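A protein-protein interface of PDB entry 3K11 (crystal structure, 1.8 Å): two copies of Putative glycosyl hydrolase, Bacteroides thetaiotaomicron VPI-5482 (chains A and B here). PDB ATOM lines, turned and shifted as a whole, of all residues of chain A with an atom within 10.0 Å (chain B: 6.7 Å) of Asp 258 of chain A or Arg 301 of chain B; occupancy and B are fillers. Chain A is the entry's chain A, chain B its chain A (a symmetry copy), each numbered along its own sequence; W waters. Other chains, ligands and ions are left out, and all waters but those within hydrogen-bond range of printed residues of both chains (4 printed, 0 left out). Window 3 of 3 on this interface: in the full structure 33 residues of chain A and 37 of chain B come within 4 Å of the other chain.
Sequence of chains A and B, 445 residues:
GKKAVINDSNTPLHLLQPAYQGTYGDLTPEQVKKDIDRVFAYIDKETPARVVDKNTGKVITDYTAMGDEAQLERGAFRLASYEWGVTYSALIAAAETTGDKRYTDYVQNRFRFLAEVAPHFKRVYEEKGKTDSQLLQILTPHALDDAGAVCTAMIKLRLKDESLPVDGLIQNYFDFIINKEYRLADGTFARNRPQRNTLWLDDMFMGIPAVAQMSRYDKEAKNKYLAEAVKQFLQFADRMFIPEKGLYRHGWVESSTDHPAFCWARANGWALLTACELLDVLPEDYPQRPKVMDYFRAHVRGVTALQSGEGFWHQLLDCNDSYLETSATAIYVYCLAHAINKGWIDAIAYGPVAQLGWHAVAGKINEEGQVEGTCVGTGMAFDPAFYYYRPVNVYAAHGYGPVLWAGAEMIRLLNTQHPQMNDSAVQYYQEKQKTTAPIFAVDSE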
ATOM      1  N   ARG A 239      18.263  33.738 -25.527  1.00  0.00           N
ATOM      2  CA  ARG A 239      18.141  32.282 -25.420  1.00  0.00           C
ATOM      3  C   ARG A 239      17.227  31.623 -26.457  1.00  0.00           C
ATOM      4  O   ARG A 239      17.505  30.524 -26.892  1.00  0.00           O
ATOM      5  CB  ARG A 239      17.590  31.943 -24.058  1.00  0.00           C
ATOM      6  CG  ARG A 239      18.544  32.376 -22.953  1.00  0.00           C
ATOM      7  CD  ARG A 239      17.870  32.186 -21.676  1.00  0.00           C
ATOM      8  NE  ARG A 239      18.694  32.342 -20.476  1.00  0.00           N
ATOM      9  CZ  ARG A 239      18.605  33.348 -19.599  1.00  0.00           C
ATOM     10  NH1 ARG A 239      17.855  34.431 -19.821  1.00  0.00           N
ATOM     11  NH2 ARG A 239      19.330  33.276 -18.498  1.00  0.00           N
ATOM     12  N   LYS A 245      17.605  30.942 -38.515  1.00  0.00           N
ATOM     13  CA  LYS A 245      16.264  30.794 -39.076  1.00  0.00           C
ATOM     14  C   LYS A 245      15.471  32.080 -39.061  1.00  0.00           C
ATOM     15  O   LYS A 245      14.488  32.234 -39.796  1.00  0.00           O
ATOM     16  CB  LYS A 245      15.490  29.732 -38.293  1.00  0.00           C
ATOM     17  CG  LYS A 245      16.078  28.336 -38.409  1.00  0.00           C
ATOM     18  CD  LYS A 245      15.284  27.245 -37.646  1.00  0.00           C
ATOM     19  CE  LYS A 245      15.582  25.792 -38.245  1.00  0.00           C
ATOM     20  NZ  LYS A 245      14.739  25.378 -39.569  1.00  0.00           N
ATOM     21  N   ARG A 249      12.385  29.551 -30.865  1.00  0.00           N
ATOM     22  CA  ARG A 249      11.946  28.273 -30.304  1.00  0.00           C
ATOM     23  C   ARG A 249      10.782  28.487 -29.300  1.00  0.00           C
ATOM     24  O   ARG A 249      10.746  29.480 -28.587  1.00  0.00           O
ATOM     25  CB  ARG A 249      13.098  27.520 -29.661  1.00  0.00           C
ATOM     26  CG  ARG A 249      13.997  28.284 -28.822  1.00  0.00           C
ATOM     27  CD  ARG A 249      15.058  27.418 -28.107  1.00  0.00           C
ATOM     28  NE  ARG A 249      16.095  26.928 -28.993  1.00  0.00           N
ATOM     29  CZ  ARG A 249      17.110  27.609 -29.508  1.00  0.00           C
ATOM     30  NH1 ARG A 249      17.293  28.889 -29.350  1.00  0.00           N
ATOM     31  NH2 ARG A 249      17.952  26.980 -30.272  1.00  0.00           N
ATOM     32  N   GLY A 251      10.240  26.685 -26.580  1.00  0.00           N
ATOM     33  CA  GLY A 251      10.687  26.459 -25.221  1.00  0.00           C
ATOM     34  C   GLY A 251      12.173  26.390 -25.038  1.00  0.00           C
ATOM     35  O   GLY A 251      12.968  26.128 -25.967  1.00  0.00           O
ATOM     36  N   TRP A 252      12.563  26.581 -23.797  1.00  0.00           N
ATOM     37  CA  TRP A 252      13.988  26.572 -23.397  1.00  0.00           C
ATOM     38  C   TRP A 252      14.074  26.130 -21.954  1.00  0.00           C
ATOM     39  O   TRP A 252      13.628  26.838 -21.071  1.00  0.00           O
ATOM     40  CB  TRP A 252      14.573  27.979 -23.530  1.00  0.00           C
ATOM     41  CG  TRP A 252      16.044  28.099 -23.316  1.00  0.00           C
ATOM     42  CD1 TRP A 252      17.039  27.999 -24.268  1.00  0.00           C
ATOM     43  CD2 TRP A 252      16.711  28.421 -22.072  1.00  0.00           C
ATOM     44  NE1 TRP A 252      18.260  28.203 -23.683  1.00  0.00           N
ATOM     45  CE2 TRP A 252      18.081  28.482 -22.343  1.00  0.00           C
ATOM     46  CE3 TRP A 252      16.257  28.674 -20.766  1.00  0.00           C
ATOM     47  CZ2 TRP A 252      19.017  28.796 -21.361  1.00  0.00           C
ATOM     48  CZ3 TRP A 252      17.187  29.004 -19.811  1.00  0.00           C
ATOM     49  CH2 TRP A 252      18.540  29.022 -20.103  1.00  0.00           C
ATOM     50  N   VAL A 253      14.696  24.976 -21.732  1.00  0.00           N
ATOM     51  CA  VAL A 253      14.884  24.434 -20.384  1.00  0.00           C
ATOM     52  C   VAL A 253      16.321  24.673 -19.952  1.00  0.00           C
ATOM     53  O   VAL A 253      17.275  24.225 -20.588  1.00  0.00           O
ATOM     54  CB  VAL A 253      14.549  22.915 -20.323  1.00  0.00           C
ATOM     55  CG1 VAL A 253      14.835  22.348 -18.913  1.00  0.00           C
ATOM     56  CG2 VAL A 253      13.035  22.724 -20.715  1.00  0.00           C
ATOM     57  N   GLU A 254      16.481  25.344 -18.836  1.00  0.00           N
ATOM     58  CA  GLU A 254      17.819  25.816 -18.445  1.00  0.00           C
ATOM     59  C   GLU A 254      18.820  24.705 -18.290  1.00  0.00           C
ATOM     60  O   GLU A 254      19.954  24.862 -18.709  1.00  0.00           O
ATOM     61  CB  GLU A 254      17.732  26.617 -17.172  1.00  0.00           C
ATOM     62  CG  GLU A 254      19.041  27.259 -16.678  1.00  0.00           C
ATOM     63  CD  GLU A 254      18.782  27.981 -15.376  1.00  0.00           C
ATOM     64  OE1 GLU A 254      18.593  27.290 -14.341  1.00  0.00           O
ATOM     65  OE2 GLU A 254      18.749  29.245 -15.405  1.00  0.00           O
ATOM     66  N   SER A 255      18.408  23.573 -17.729  1.00  0.00           N
ATOM     67  CA  SER A 255      19.352  22.477 -17.499  1.00  0.00           C
ATOM     68  C   SER A 255      19.798  21.727 -18.739  1.00  0.00           C
ATOM     69  O   SER A 255      20.822  21.009 -18.709  1.00  0.00           O
ATOM     70  CB  SER A 255      18.786  21.458 -16.539  1.00  0.00           C
ATOM     71  OG  SER A 255      17.715  20.702 -17.094  1.00  0.00           O
ATOM     72  N   SER A 256      19.038  21.839 -19.809  1.00  0.00           N
ATOM     73  CA  SER A 256      19.330  21.043 -21.001  1.00  0.00           C
ATOM     74  C   SER A 256      20.587  21.513 -21.731  1.00  0.00           C
ATOM     75  O   SER A 256      20.797  22.700 -21.920  1.00  0.00           O
ATOM     76  CB  SER A 256      18.145  21.000 -21.978  1.00  0.00           C
ATOM     77  OG  SER A 256      17.054  20.248 -21.464  1.00  0.00           O
ATOM     78  N   THR A 257      21.402  20.570 -22.181  1.00  0.00           N
ATOM     79  CA  THR A 257      22.655  20.903 -22.811  1.00  0.00           C
ATOM     80  C   THR A 257      22.486  21.233 -24.290  1.00  0.00           C
ATOM     81  O   THR A 257      23.378  21.804 -24.890  1.00  0.00           O
ATOM     82  CB  THR A 257      23.705  19.778 -22.575  1.00  0.00           C
ATOM     83  OG1 THR A 257      23.133  18.531 -22.967  1.00  0.00           O
ATOM     84  CG2 THR A 257      24.100  19.674 -21.062  1.00  0.00           C
ATOM     85  N   ASP A 258      21.366  20.841 -24.890  1.00  0.00           N
ATOM     86  CA  ASP A 258      20.946  21.261 -26.224  1.00  0.00           C
ATOM     87  C   ASP A 258      19.544  21.782 -26.043  1.00  0.00           C
ATOM     88  O   ASP A 258      18.849  21.393 -25.101  1.00  0.00           O
ATOM     89  CB  ASP A 258      20.863  20.080 -27.185  1.00  0.00           C
ATOM     90  CG  ASP A 258      22.171  19.713 -27.805  1.00  0.00           C
ATOM     91  OD1 ASP A 258      23.175  20.414 -27.636  1.00  0.00           O
ATOM     92  OD2 ASP A 258      22.187  18.700 -28.509  1.00  0.00           O
ATOM     93  N   HIS A 259      19.128  22.695 -26.925  1.00  0.00           N
ATOM     94  CA  HIS A 259      17.832  23.331 -26.832  1.00  0.00           C
ATOM     95  C   HIS A 259      17.076  23.169 -28.126  1.00  0.00           C
ATOM     96  O   HIS A 259      17.042  24.071 -28.940  1.00  0.00           O
ATOM     97  CB  HIS A 259      17.992  24.814 -26.461  1.00  0.00           C
ATOM     98  CG  HIS A 259      18.716  25.024 -25.166  1.00  0.00           C
ATOM     99  ND1 HIS A 259      18.170  24.671 -23.948  1.00  0.00           N
ATOM    100  CD2 HIS A 259      19.935  25.560 -24.900  1.00  0.00           C
ATOM    101  CE1 HIS A 259      19.045  24.943 -22.995  1.00  0.00           C
ATOM    102  NE2 HIS A 259      20.122  25.492 -23.542  1.00  0.00           N
ATOM    103  N   PRO A 260      16.405  22.023 -28.299  1.00  0.00           N
ATOM    104  CA  PRO A 260      15.659  21.751 -29.547  1.00  0.00           C
ATOM    105  C   PRO A 260      14.632  22.821 -29.867  1.00  0.00           C
ATOM    106  O   PRO A 260      14.039  23.413 -28.973  1.00  0.00           O
ATOM    107  CB  PRO A 260      14.957  20.429 -29.245  1.00  0.00           C
ATOM    108  CG  PRO A 260      15.786  19.766 -28.195  1.00  0.00           C
ATOM    109  CD  PRO A 260      16.259  20.911 -27.327  1.00  0.00           C
ATOM    110  N   ALA A 261      14.473  23.115 -31.156  1.00  0.00           N
ATOM    111  CA  ALA A 261      13.611  24.183 -31.613  1.00  0.00           C
ATOM    112  C   ALA A 261      12.360  23.591 -32.227  1.00  0.00           C
ATOM    113  O   ALA A 261      12.446  22.837 -33.184  1.00  0.00           O
ATOM    114  CB  ALA A 261      14.340  25.033 -32.650  1.00  0.00           C
ATOM    115  N   PHE A 262      11.220  23.889 -31.631  1.00  0.00           N
ATOM    116  CA  PHE A 262       9.949  23.664 -32.244  1.00  0.00           C
ATOM    117  C   PHE A 262       9.367  25.065 -32.435  1.00  0.00           C
ATOM    118  O   PHE A 262       8.980  25.714 -31.475  1.00  0.00           O
ATOM    119  CB  PHE A 262       9.087  22.758 -31.381  1.00  0.00           C
ATOM    120  CG  PHE A 262       9.636  21.336 -31.326  1.00  0.00           C
ATOM    121  CD1 PHE A 262       9.331  20.441 -32.332  1.00  0.00           C
ATOM    122  CD2 PHE A 262      10.511  20.966 -30.356  1.00  0.00           C
ATOM    123  CE1 PHE A 262       9.911  19.207 -32.363  1.00  0.00           C
ATOM    124  CE2 PHE A 262      11.060  19.686 -30.371  1.00  0.00           C
ATOM    125  CZ  PHE A 262      10.753  18.837 -31.380  1.00  0.00           C
ATOM    126  N   PHE A 382       8.870  18.256 -26.613  1.00  0.00           N
ATOM    127  CA  PHE A 382      10.141  18.051 -27.255  1.00  0.00           C
ATOM    128  C   PHE A 382      10.086  16.957 -28.331  1.00  0.00           C
ATOM    129  O   PHE A 382      11.049  16.256 -28.602  1.00  0.00           O
ATOM    130  CB  PHE A 382      11.232  17.818 -26.206  1.00  0.00           C
ATOM    131  CG  PHE A 382      11.508  19.044 -25.433  1.00  0.00           C
ATOM    132  CD1 PHE A 382      12.114  20.124 -26.053  1.00  0.00           C
ATOM    133  CD2 PHE A 382      11.080  19.181 -24.149  1.00  0.00           C
ATOM    134  CE1 PHE A 382      12.296  21.311 -25.388  1.00  0.00           C
ATOM    135  CE2 PHE A 382      11.271  20.343 -23.497  1.00  0.00           C
ATOM    136  CZ  PHE A 382      11.892  21.393 -24.100  1.00  0.00           C
ATOM    137  N   LYS B 245      24.231  21.554 -42.380  1.00  0.00           N
ATOM    138  CA  LYS B 245      23.020  20.757 -42.187  1.00  0.00           C
ATOM    139  C   LYS B 245      23.074  19.891 -40.950  1.00  0.00           C
ATOM    140  O   LYS B 245      22.041  19.439 -40.442  1.00  0.00           O
ATOM    141  CB  LYS B 245      22.791  19.861 -43.404  1.00  0.00           C
ATOM    142  CG  LYS B 245      22.510  20.629 -44.685  1.00  0.00           C
ATOM    143  CD  LYS B 245      22.243  19.731 -45.920  1.00  0.00           C
ATOM    144  CE  LYS B 245      21.419  20.522 -47.040  1.00  0.00           C
ATOM    145  NZ  LYS B 245      19.811  20.587 -46.832  1.00  0.00           N
ATOM    146  N   GLY B 246      24.275  19.613 -40.485  1.00  0.00           N
ATOM    147  CA  GLY B 246      24.426  18.627 -39.421  1.00  0.00           C
ATOM    148  C   GLY B 246      24.109  17.222 -39.878  1.00  0.00           C
ATOM    149  O   GLY B 246      23.681  16.418 -39.071  1.00  0.00           O
ATOM    150  N   LEU B 247      24.395  16.917 -41.146  1.00  0.00           N
ATOM    151  CA  LEU B 247      24.077  15.635 -41.761  1.00  0.00           C
ATOM    152  C   LEU B 247      25.277  15.210 -42.599  1.00  0.00           C
ATOM    153  O   LEU B 247      26.157  16.021 -42.906  1.00  0.00           O
ATOM    154  CB  LEU B 247      22.833  15.784 -42.683  1.00  0.00           C
ATOM    155  CG  LEU B 247      21.525  16.275 -42.091  1.00  0.00           C
ATOM    156  CD1 LEU B 247      20.498  16.406 -43.260  1.00  0.00           C
ATOM    157  CD2 LEU B 247      21.052  15.324 -40.995  1.00  0.00           C
ATOM    158  N   ASP B 294      32.229  15.816 -30.573  1.00  0.00           N
ATOM    159  CA  ASP B 294      31.706  16.979 -31.281  1.00  0.00           C
ATOM    160  C   ASP B 294      30.985  16.612 -32.591  1.00  0.00           C
ATOM    161  O   ASP B 294      29.920  17.154 -32.870  1.00  0.00           O
ATOM    162  CB  ASP B 294      32.831  17.962 -31.595  1.00  0.00           C
ATOM    163  CG  ASP B 294      33.339  18.708 -30.356  1.00  0.00           C
ATOM    164  OD1 ASP B 294      32.730  18.612 -29.262  1.00  0.00           O
ATOM    165  OD2 ASP B 294      34.382  19.373 -30.496  1.00  0.00           O
ATOM    166  N   PHE B 296      29.652  13.684 -33.238  1.00  0.00           N
ATOM    167  CA  PHE B 296      28.425  12.966 -32.808  1.00  0.00           C
ATOM    168  C   PHE B 296      27.333  13.917 -32.379  1.00  0.00           C
ATOM    169  O   PHE B 296      26.206  13.879 -32.879  1.00  0.00           O
ATOM    170  CB  PHE B 296      28.729  12.068 -31.614  1.00  0.00           C
ATOM    171  CG  PHE B 296      27.505  11.313 -31.111  1.00  0.00           C
ATOM    172  CD1 PHE B 296      26.834  10.412 -31.941  1.00  0.00           C
ATOM    173  CD2 PHE B 296      27.007  11.570 -29.839  1.00  0.00           C
ATOM    174  CE1 PHE B 296      25.666   9.780 -31.508  1.00  0.00           C
ATOM    175  CE2 PHE B 296      25.844  10.932 -29.373  1.00  0.00           C
ATOM    176  CZ  PHE B 296      25.188  10.027 -30.205  1.00  0.00           C
ATOM    177  N   ARG B 297      27.679  14.829 -31.489  1.00  0.00           N
ATOM    178  CA  ARG B 297      26.705  15.808 -31.050  1.00  0.00           C
ATOM    179  C   ARG B 297      26.124  16.694 -32.158  1.00  0.00           C
ATOM    180  O   ARG B 297      24.920  16.998 -32.139  1.00  0.00           O
ATOM    181  CB  ARG B 297      27.279  16.625 -29.913  1.00  0.00           C
ATOM    182  CG  ARG B 297      27.333  15.845 -28.610  1.00  0.00           C
ATOM    183  CD  ARG B 297      27.915  16.700 -27.545  1.00  0.00           C
ATOM    184  NE  ARG B 297      27.830  15.939 -26.292  1.00  0.00           N
ATOM    185  CZ  ARG B 297      28.732  15.971 -25.319  1.00  0.00           C
ATOM    186  NH1 ARG B 297      29.802  16.777 -25.398  1.00  0.00           N
ATOM    187  NH2 ARG B 297      28.573  15.181 -24.256  1.00  0.00           N
ATOM    188  N   ALA B 298      26.943  17.127 -33.117  1.00  0.00           N
ATOM    189  CA  ALA B 298      26.468  17.925 -34.238  1.00  0.00           C
ATOM    190  C   ALA B 298      25.516  17.109 -35.116  1.00  0.00           C
ATOM    191  O   ALA B 298      24.512  17.628 -35.596  1.00  0.00           O
ATOM    192  CB  ALA B 298      27.629  18.459 -35.088  1.00  0.00           C
ATOM    193  N   HIS B 299      25.814  15.825 -35.304  1.00  0.00           N
ATOM    194  CA  HIS B 299      24.957  14.950 -36.102  1.00  0.00           C
ATOM    195  C   HIS B 299      23.618  14.692 -35.412  1.00  0.00           C
ATOM    196  O   HIS B 299      22.554  14.715 -36.032  1.00  0.00           O
ATOM    197  CB  HIS B 299      25.688  13.639 -36.376  1.00  0.00           C
ATOM    198  CG  HIS B 299      25.088  12.825 -37.477  1.00  0.00           C
ATOM    199  ND1 HIS B 299      25.291  11.465 -37.578  1.00  0.00           N
ATOM    200  CD2 HIS B 299      24.284  13.171 -38.517  1.00  0.00           C
ATOM    201  CE1 HIS B 299      24.664  11.014 -38.655  1.00  0.00           C
ATOM    202  NE2 HIS B 299      24.047  12.023 -39.247  1.00  0.00           N
ATOM    203  N   VAL B 300      23.669  14.527 -34.103  1.00  0.00           N
ATOM    204  CA  VAL B 300      22.441  14.371 -33.319  1.00  0.00           C
ATOM    205  C   VAL B 300      21.507  15.574 -33.549  1.00  0.00           C
ATOM    206  O   VAL B 300      20.286  15.409 -33.805  1.00  0.00           O
ATOM    207  CB  VAL B 300      22.716  14.180 -31.833  1.00  0.00           C
ATOM    208  CG1 VAL B 300      21.443  14.434 -30.982  1.00  0.00           C
ATOM    209  CG2 VAL B 300      23.264  12.806 -31.540  1.00  0.00           C
ATOM    210  N   ARG B 301      22.060  16.778 -33.451  1.00  0.00           N
ATOM    211  CA  ARG B 301      21.259  17.972 -33.627  1.00  0.00           C
ATOM    212  C   ARG B 301      20.651  18.084 -35.033  1.00  0.00           C
ATOM    213  O   ARG B 301      19.512  18.532 -35.177  1.00  0.00           O
ATOM    214  CB  ARG B 301      22.070  19.226 -33.274  1.00  0.00           C
ATOM    215  CG  ARG B 301      22.326  19.379 -31.783  1.00  0.00           C
ATOM    216  CD  ARG B 301      22.904  20.755 -31.462  1.00  0.00           C
ATOM    217  NE  ARG B 301      24.292  20.881 -31.873  1.00  0.00           N
ATOM    218  CZ  ARG B 301      25.345  20.520 -31.129  1.00  0.00           C
ATOM    219  NH1 ARG B 301      25.217  19.968 -29.916  1.00  0.00           N
ATOM    220  NH2 ARG B 301      26.557  20.664 -31.626  1.00  0.00           N
ATOM    221  N   GLY B 302      21.411  17.717 -36.059  1.00  0.00           N
ATOM    222  CA  GLY B 302      20.924  17.795 -37.452  1.00  0.00           C
ATOM    223  C   GLY B 302      19.876  16.769 -37.760  1.00  0.00           C
ATOM    224  O   GLY B 302      18.897  17.071 -38.409  1.00  0.00           O
ATOM    225  N   VAL B 303      20.087  15.543 -37.309  1.00  0.00           N
ATOM    226  CA  VAL B 303      19.126  14.462 -37.530  1.00  0.00           C
ATOM    227  C   VAL B 303      17.824  14.733 -36.798  1.00  0.00           C
ATOM    228  O   VAL B 303      16.733  14.643 -37.387  1.00  0.00           O
ATOM    229  CB  VAL B 303      19.699  13.048 -37.132  1.00  0.00           C
ATOM    230  CG1 VAL B 303      18.552  11.971 -37.087  1.00  0.00           C
ATOM    231  CG2 VAL B 303      20.864  12.635 -38.110  1.00  0.00           C
ATOM    232  N   THR B 304      17.900  15.072 -35.508  1.00  0.00           N
ATOM    233  CA  THR B 304      16.703  15.133 -34.708  1.00  0.00           C
ATOM    234  C   THR B 304      15.797  16.255 -35.168  1.00  0.00           C
ATOM    235  O   THR B 304      14.597  16.115 -35.111  1.00  0.00           O
ATOM    236  CB  THR B 304      16.998  15.296 -33.248  1.00  0.00           C
ATOM    237  OG1 THR B 304      17.888  16.406 -33.065  1.00  0.00           O
ATOM    238  CG2 THR B 304      17.653  14.029 -32.662  1.00  0.00           C
ATOM    239  N   ALA B 305      16.369  17.346 -35.655  1.00  0.00           N
ATOM    240  CA  ALA B 305      15.564  18.480 -36.150  1.00  0.00           C
ATOM    241  C   ALA B 305      14.662  18.067 -37.299  1.00  0.00           C
ATOM    242  O   ALA B 305      13.701  18.770 -37.586  1.00  0.00           O
ATOM    243  CB  ALA B 305      16.463  19.609 -36.598  1.00  0.00           C
ATOM    244  N   LEU B 306      15.015  16.988 -38.007  1.00  0.00           N
ATOM    245  CA  LEU B 306      14.247  16.579 -39.181  1.00  0.00           C
ATOM    246  C   LEU B 306      13.306  15.398 -38.948  1.00  0.00           C
ATOM    247  O   LEU B 306      12.740  14.848 -39.900  1.00  0.00           O
ATOM    248  CB  LEU B 306      15.209  16.296 -40.321  1.00  0.00           C
ATOM    249  CG  LEU B 306      16.010  17.544 -40.753  1.00  0.00           C
ATOM    250  CD1 LEU B 306      17.206  17.099 -41.693  1.00  0.00           C
ATOM    251  CD2 LEU B 306      15.076  18.596 -41.420  1.00  0.00           C
ATOM    252  N   ILE B 345      24.090  12.850 -24.298  1.00  0.00           N
ATOM    253  CA  ILE B 345      23.110  13.873 -24.673  1.00  0.00           C
ATOM    254  C   ILE B 345      22.018  13.958 -23.629  1.00  0.00           C
ATOM    255  O   ILE B 345      21.852  13.108 -22.763  1.00  0.00           O
ATOM    256  CB  ILE B 345      22.548  13.627 -26.137  1.00  0.00           C
ATOM    257  CG1 ILE B 345      21.557  12.441 -26.178  1.00  0.00           C
ATOM    258  CG2 ILE B 345      23.690  13.522 -27.178  1.00  0.00           C
ATOM    259  CD1 ILE B 345      20.969  12.104 -27.584  1.00  0.00           C
ATOM    260  N   ASP B 346      21.299  15.065 -23.681  1.00  0.00           N
ATOM    261  CA  ASP B 346      20.339  15.431 -22.677  1.00  0.00           C
ATOM    262  C   ASP B 346      19.032  14.670 -22.733  1.00  0.00           C
ATOM    263  O   ASP B 346      18.391  14.546 -23.786  1.00  0.00           O
ATOM    264  CB  ASP B 346      20.061  16.923 -22.847  1.00  0.00           C
ATOM    265  CG  ASP B 346      19.309  17.509 -21.708  1.00  0.00           C
ATOM    266  OD1 ASP B 346      19.915  17.755 -20.614  1.00  0.00           O
ATOM    267  OD2 ASP B 346      18.105  17.741 -21.928  1.00  0.00           O
ATOM    268  N   ALA B 349      15.754  16.906 -23.467  1.00  0.00           N
ATOM    269  CA  ALA B 349      15.692  17.288 -24.870  1.00  0.00           C
ATOM    270  C   ALA B 349      15.406  16.137 -25.828  1.00  0.00           C
ATOM    271  O   ALA B 349      14.662  16.308 -26.786  1.00  0.00           O
ATOM    272  CB  ALA B 349      16.986  18.031 -25.307  1.00  0.00           C
ATOM    273  N   TYR B 350      16.009  14.973 -25.579  1.00  0.00           N
ATOM    274  CA  TYR B 350      15.957  13.895 -26.539  1.00  0.00           C
ATOM    275  C   TYR B 350      15.115  12.687 -26.179  1.00  0.00           C
ATOM    276  O   TYR B 350      14.806  11.893 -27.041  1.00  0.00           O
ATOM    277  CB  TYR B 350      17.389  13.488 -26.949  1.00  0.00           C
ATOM    278  CG  TYR B 350      18.099  14.622 -27.654  1.00  0.00           C
ATOM    279  CD1 TYR B 350      17.641  15.107 -28.876  1.00  0.00           C
ATOM    280  CD2 TYR B 350      19.201  15.265 -27.064  1.00  0.00           C
ATOM    281  CE1 TYR B 350      18.264  16.151 -29.495  1.00  0.00           C
ATOM    282  CE2 TYR B 350      19.826  16.363 -27.698  1.00  0.00           C
ATOM    283  CZ  TYR B 350      19.358  16.778 -28.922  1.00  0.00           C
ATOM    284  OH  TYR B 350      19.973  17.833 -29.607  1.00  0.00           O
HETATM  285  O   HOH W   1      18.782  18.360 -18.260  1.00  0.00           O
HETATM  286  O   HOH W   2      23.895  16.806 -29.454  1.00  0.00           O
HETATM  287  O   HOH W   3      22.352  17.221 -25.347  1.00  0.00           O
HETATM  288  O   HOH W   4      13.474  17.556 -28.960  1.00  0.00           O
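Position printed for both chains: 245.
OG of Ser 256 of chain A is in hydrogen-bond range of OD2 of Asp 346 of chain B (2.8 Å).
NH1 of Arg 301 of chain B lies within salt-bridge range of OD1 of Asp 258 of chain A, 3.1 Å away.
OD2 of Asp 258 of chain A is in hydrogen-bond range of OH of Tyr 350 of chain B.
Hydrophobic or aromatic side chains of chain B that line the printed part of chain A: Ala 349 and Tyr 350.
Along chain B the printed residues that touch a printed residue of chain A span positions 301 to 350.
Hydrophobic or aromatic side chains of chain A that line the printed part of chain B: Pro 260 and Phe 382.
The backbone carbonyl oxygen of Ser 256 of chain A lies close to a ring nitrogen (NE2) of His 259 of chain A (3.3 Å).
The backbone carbonyl oxygen (O) of Arg 301 of chain B sits at hydrogen-bond distance from the side-chain hydroxyl (OG1) of Thr 304 of chain B.
OD2 of Asp 346 of chain B lies within hydrogen-bond range of N of Ala 349 of chain B.
Water W1 lies within hydrogen-bond range of OD1 of Asp 346 of chain B (2.7 Å) and OG of Ser 255 of chain A (2.8 Å).
Water W2 lies within hydrogen-bond range of the side-chain carboxylate (OD2) of Asp 258 of chain A (2.7 Å), the backbone carbonyl oxygen (O) of Arg 297 of chain B (2.9 Å) and the guanidinium group (NH1) of Arg 301 of chain B (3.5 Å).
Water W4 lies within hydrogen-bond range of O of Ala 349 of chain B (2.8 Å) and O of Phe 382 of chain A (2.8 Å).
Water W3 lies within hydrogen-bond range of OG1 of Thr 257 of chain A (2.8 Å), N of Asp 346 of chain B (2.9 Å) and OD2 of Asp 258 of chain A (3.5 Å).
Of the printed residues of chain B, Asp 258 of chain A touches Arg 301, Ala 349 and Tyr 350.
Printed residues of chain A within 4 Å of Arg 301 of chain B: Asp 258 (3.1 Å).
No residue of chain A comes within 4 Å of Ala 298 of chain B.
No residue of chain A comes within 4 Å of Val 300 of chain B.
No residue of chain A comes within 4 Å of Gly 302 of chain B.
No residue of chain A comes within 4 Å of Thr 304 of chain B.
Of the printed residues of chain B, Ser 256 of chain A touches Asp 346 (2.8 Å).
Printed residues of chain A within 4 Å of Tyr 350 of chain B: Asp 258 (2.6 Å).
Of the printed residues of chain B, Thr 257 of chain A touches Asp 346 (3.5 Å).
Printed residues of chain A within 4 Å of Asp 346 of chain B: Ser 255, Ser 256 and Thr 257.
Ser 255 of chain A touches Asp 346 of chain B (O to OD1, 3.9 Å).
Thr 257 of chain A touches Asp 346 of chain B.
O of Asp 258 of chain A touches CB of Ala 349 of chain B, at 3.8 Å.
Pro 260 of chain A touches Ala 349 of chain B.
CB of Phe 382 of chain A touches O of Ala 349 of chain B, at 3.8 Å.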
